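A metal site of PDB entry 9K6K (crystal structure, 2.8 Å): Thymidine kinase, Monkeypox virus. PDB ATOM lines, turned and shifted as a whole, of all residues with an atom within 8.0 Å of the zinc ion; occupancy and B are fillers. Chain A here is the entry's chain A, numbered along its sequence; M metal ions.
The nearest printed residue that does not touch the zinc ion is Lys 143 (4.3 Å).
SG of Cys 170 lies close to N of Lys 172, 3.7 Å away.
O of Lys 143 lies within hydrogen-bond range of N of Cys 138, 2.5 Å away.
The side-chain sulfur of Cys 138 lies close to the backbone NH of Lys 140 (3.5 Å).
The zinc ion is bound by SG of Cys 141, at 2.1 Å.
The side-chain sulfur (SG) of Cys 173 binds the zinc ion, at 2.3 Å.
The zinc ion is bound by SG of Cys 170 (2.5 Å).
The zinc ion is bound by SG of Cys 138, at 2.6 Å.
The zinc ion has four donor atoms within binding distance.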
ATOM      1  N   VAL A 137      -1.467   9.212  -1.228  1.00  0.00           N
ATOM      2  CA  VAL A 137      -0.099   9.330  -1.719  1.00  0.00           C
ATOM      3  C   VAL A 137       0.833   9.450  -0.515  1.00  0.00           C
ATOM      4  O   VAL A 137       0.543  10.200   0.422  1.00  0.00           O
ATOM      5  CB  VAL A 137       0.065  10.531  -2.674  1.00  0.00           C
ATOM      6  CG1 VAL A 137       1.505  10.656  -3.125  1.00  0.00           C
ATOM      7  CG2 VAL A 137      -0.842  10.351  -3.878  1.00  0.00           C
ATOM      8  N   CYS A 138       1.913   8.681  -0.515  1.00  0.00           N
ATOM      9  CA  CYS A 138       2.825   8.697   0.619  1.00  0.00           C
ATOM     10  C   CYS A 138       3.525  10.044   0.742  1.00  0.00           C
ATOM     11  O   CYS A 138       4.014  10.594  -0.247  1.00  0.00           O
ATOM     12  CB  CYS A 138       3.854   7.574   0.517  1.00  0.00           C
ATOM     13  SG  CYS A 138       4.865   7.467   1.998  1.00  0.00           S
ATOM     14  N   MET A 139       3.548  10.584   1.951  1.00  0.00           N
ATOM     15  CA  MET A 139       4.175  11.870   2.212  1.00  0.00           C
ATOM     16  C   MET A 139       5.665  11.777   2.524  1.00  0.00           C
ATOM     17  O   MET A 139       6.262  12.781   2.912  1.00  0.00           O
ATOM     18  CB  MET A 139       3.427  12.578   3.344  1.00  0.00           C
ATOM     19  CG  MET A 139       1.990  12.940   2.992  1.00  0.00           C
ATOM     20  SD  MET A 139       1.055  13.633   4.367  1.00  0.00           S
ATOM     21  CE  MET A 139      -0.544  13.848   3.607  1.00  0.00           C
ATOM     22  N   LYS A 140       6.280  10.606   2.363  1.00  0.00           N
ATOM     23  CA  LYS A 140       7.721  10.451   2.564  1.00  0.00           C
ATOM     24  C   LYS A 140       8.458  10.034   1.304  1.00  0.00           C
ATOM     25  O   LYS A 140       9.450  10.664   0.942  1.00  0.00           O
ATOM     26  CB  LYS A 140       8.003   9.447   3.701  1.00  0.00           C
ATOM     27  CG  LYS A 140       7.483   9.890   5.061  1.00  0.00           C
ATOM     28  CD  LYS A 140       8.129   9.107   6.192  1.00  0.00           C
ATOM     29  CE  LYS A 140       7.757   9.718   7.546  1.00  0.00           C
ATOM     30  NZ  LYS A 140       8.457   9.055   8.681  1.00  0.00           N
ATOM     31  N   CYS A 141       8.010   8.964   0.638  1.00  0.00           N
ATOM     32  CA  CYS A 141       8.632   8.495  -0.599  1.00  0.00           C
ATOM     33  C   CYS A 141       7.694   8.625  -1.794  1.00  0.00           C
ATOM     34  O   CYS A 141       7.918   7.972  -2.822  1.00  0.00           O
ATOM     35  CB  CYS A 141       9.043   7.038  -0.441  1.00  0.00           C
ATOM     36  SG  CYS A 141       7.576   6.002  -0.442  1.00  0.00           S
ATOM     37  N   PHE A 142       6.660   9.447  -1.683  1.00  0.00           N
ATOM     38  CA  PHE A 142       5.726   9.777  -2.756  1.00  0.00           C
ATOM     39  C   PHE A 142       5.225   8.597  -3.597  1.00  0.00           C
ATOM     40  O   PHE A 142       5.095   8.732  -4.815  1.00  0.00           O
ATOM     41  CB  PHE A 142       6.375  10.798  -3.679  1.00  0.00           C
ATOM     42  CG  PHE A 142       6.835  12.051  -2.986  1.00  0.00           C
ATOM     43  CD1 PHE A 142       5.932  12.992  -2.537  1.00  0.00           C
ATOM     44  CD2 PHE A 142       8.191  12.283  -2.779  1.00  0.00           C
ATOM     45  CE1 PHE A 142       6.354  14.144  -1.899  1.00  0.00           C
ATOM     46  CE2 PHE A 142       8.621  13.423  -2.143  1.00  0.00           C
ATOM     47  CZ  PHE A 142       7.703  14.358  -1.703  1.00  0.00           C
ATOM     48  N   LYS A 143       4.942   7.441  -2.984  1.00  0.00           N
ATOM     49  CA  LYS A 143       4.281   6.349  -3.688  1.00  0.00           C
ATOM     50  C   LYS A 143       2.900   6.123  -3.064  1.00  0.00           C
ATOM     51  O   LYS A 143       2.409   6.949  -2.289  1.00  0.00           O
ATOM     52  CB  LYS A 143       5.162   5.104  -3.677  1.00  0.00           C
ATOM     53  CG  LYS A 143       5.248   4.371  -2.355  1.00  0.00           C
ATOM     54  CD  LYS A 143       6.446   3.413  -2.355  1.00  0.00           C
ATOM     55  CE  LYS A 143       6.787   2.917  -3.752  1.00  0.00           C
ATOM     56  NZ  LYS A 143       8.179   2.388  -3.829  1.00  0.00           N
ATOM     57  N   GLU A 144       2.249   5.017  -3.424  1.00  0.00           N
ATOM     58  CA  GLU A 144       0.895   4.780  -2.918  1.00  0.00           C
ATOM     59  C   GLU A 144       0.907   4.576  -1.402  1.00  0.00           C
ATOM     60  O   GLU A 144       1.770   3.895  -0.857  1.00  0.00           O
ATOM     61  CB  GLU A 144       0.261   3.576  -3.597  1.00  0.00           C
ATOM     62  CG  GLU A 144      -0.086   3.786  -5.056  1.00  0.00           C
ATOM     63  CD  GLU A 144      -0.752   2.577  -5.680  1.00  0.00           C
ATOM     64  OE1 GLU A 144      -1.349   2.719  -6.768  1.00  0.00           O
ATOM     65  OE2 GLU A 144      -0.684   1.479  -5.078  1.00  0.00           O
ATOM     66  N   ALA A 145      -0.084   5.185  -0.731  1.00  0.00           N
ATOM     67  CA  ALA A 145      -0.242   5.106   0.715  1.00  0.00           C
ATOM     68  C   ALA A 145      -1.566   4.434   1.056  1.00  0.00           C
ATOM     69  O   ALA A 145      -2.582   4.667   0.395  1.00  0.00           O
ATOM     70  CB  ALA A 145      -0.170   6.491   1.345  1.00  0.00           C
ATOM     71  N   SER A 168      -0.408  10.293   5.742  1.00  0.00           N
ATOM     72  CA  SER A 168      -0.708   9.059   5.034  1.00  0.00           C
ATOM     73  C   SER A 168       0.601   8.466   4.515  1.00  0.00           C
ATOM     74  O   SER A 168       1.344   9.137   3.791  1.00  0.00           O
ATOM     75  CB  SER A 168      -1.697   9.315   3.891  1.00  0.00           C
ATOM     76  OG  SER A 168      -1.155  10.222   2.952  1.00  0.00           O
ATOM     77  N   VAL A 169       0.877   7.211   4.891  1.00  0.00           N
ATOM     78  CA  VAL A 169       2.137   6.568   4.558  1.00  0.00           C
ATOM     79  C   VAL A 169       1.863   5.184   3.972  1.00  0.00           C
ATOM     80  O   VAL A 169       0.748   4.658   4.049  1.00  0.00           O
ATOM     81  CB  VAL A 169       3.071   6.448   5.776  1.00  0.00           C
ATOM     82  CG1 VAL A 169       3.572   7.821   6.190  1.00  0.00           C
ATOM     83  CG2 VAL A 169       2.350   5.775   6.933  1.00  0.00           C
ATOM     84  N   CYS A 170       2.918   4.613   3.416  1.00  0.00           N
ATOM     85  CA  CYS A 170       2.925   3.273   2.859  1.00  0.00           C
ATOM     86  C   CYS A 170       3.458   2.288   3.905  1.00  0.00           C
ATOM     87  O   CYS A 170       3.686   2.639   5.069  1.00  0.00           O
ATOM     88  CB  CYS A 170       3.762   3.245   1.584  1.00  0.00           C
ATOM     89  SG  CYS A 170       5.518   3.568   1.877  1.00  0.00           S
ATOM     90  N   ARG A 171       3.689   1.054   3.486  1.00  0.00           N
ATOM     91  CA  ARG A 171       4.135   0.046   4.442  1.00  0.00           C
ATOM     92  C   ARG A 171       5.588   0.260   4.845  1.00  0.00           C
ATOM     93  O   ARG A 171       5.925   0.173   6.033  1.00  0.00           O
ATOM     94  CB  ARG A 171       3.941  -1.349   3.851  1.00  0.00           C
ATOM     95  CG  ARG A 171       4.304  -2.438   4.813  1.00  0.00           C
ATOM     96  CD  ARG A 171       4.007  -3.795   4.233  1.00  0.00           C
ATOM     97  NE  ARG A 171       3.136  -4.555   5.121  1.00  0.00           N
ATOM     98  CZ  ARG A 171       1.819  -4.665   4.951  1.00  0.00           C
ATOM     99  NH1 ARG A 171       1.225  -4.050   3.936  1.00  0.00           N
ATOM    100  NH2 ARG A 171       1.101  -5.383   5.808  1.00  0.00           N
ATOM    101  N   LYS A 172       6.447   0.560   3.877  1.00  0.00           N
ATOM    102  CA  LYS A 172       7.866   0.728   4.169  1.00  0.00           C
ATOM    103  C   LYS A 172       8.105   1.946   5.069  1.00  0.00           C
ATOM    104  O   LYS A 172       8.924   1.886   5.996  1.00  0.00           O
ATOM    105  CB  LYS A 172       8.648   0.873   2.861  1.00  0.00           C
ATOM    106  CG  LYS A 172      10.143   0.987   3.021  1.00  0.00           C
ATOM    107  CD  LYS A 172      10.763   1.336   1.681  1.00  0.00           C
ATOM    108  CE  LYS A 172      10.169   2.647   1.170  1.00  0.00           C
ATOM    109  NZ  LYS A 172      10.690   3.086  -0.153  1.00  0.00           N
ATOM    110  N   CYS A 173       7.378   3.038   4.822  1.00  0.00           N
ATOM    111  CA  CYS A 173       7.550   4.262   5.591  1.00  0.00           C
ATOM    112  C   CYS A 173       6.839   4.240   6.931  1.00  0.00           C
ATOM    113  O   CYS A 173       7.139   5.079   7.800  1.00  0.00           O
ATOM    114  CB  CYS A 173       7.046   5.453   4.787  1.00  0.00           C
ATOM    115  SG  CYS A 173       8.003   5.779   3.317  1.00  0.00           S
ATOM    116  N   TYR A 174       5.921   3.298   7.134  1.00  0.00           N
ATOM    117  CA  TYR A 174       5.224   3.213   8.414  1.00  0.00           C
ATOM    118  C   TYR A 174       6.094   2.569   9.482  1.00  0.00           C
ATOM    119  O   TYR A 174       6.005   2.945  10.661  1.00  0.00           O
ATOM    120  CB  TYR A 174       3.926   2.421   8.248  1.00  0.00           C
ATOM    121  CG  TYR A 174       3.090   2.345   9.511  1.00  0.00           C
ATOM    122  CD1 TYR A 174       2.189   3.357   9.824  1.00  0.00           C
ATOM    123  CD2 TYR A 174       3.206   1.269  10.382  1.00  0.00           C
ATOM    124  CE1 TYR A 174       1.419   3.291  10.976  1.00  0.00           C
ATOM    125  CE2 TYR A 174       2.445   1.200  11.532  1.00  0.00           C
ATOM    126  CZ  TYR A 174       1.550   2.212  11.824  1.00  0.00           C
ATOM    127  OH  TYR A 174       0.787   2.144  12.964  1.00  0.00           O
HETATM  128 ZN    ZN M   1       6.657   5.701   1.453  1.00  0.00          ZN
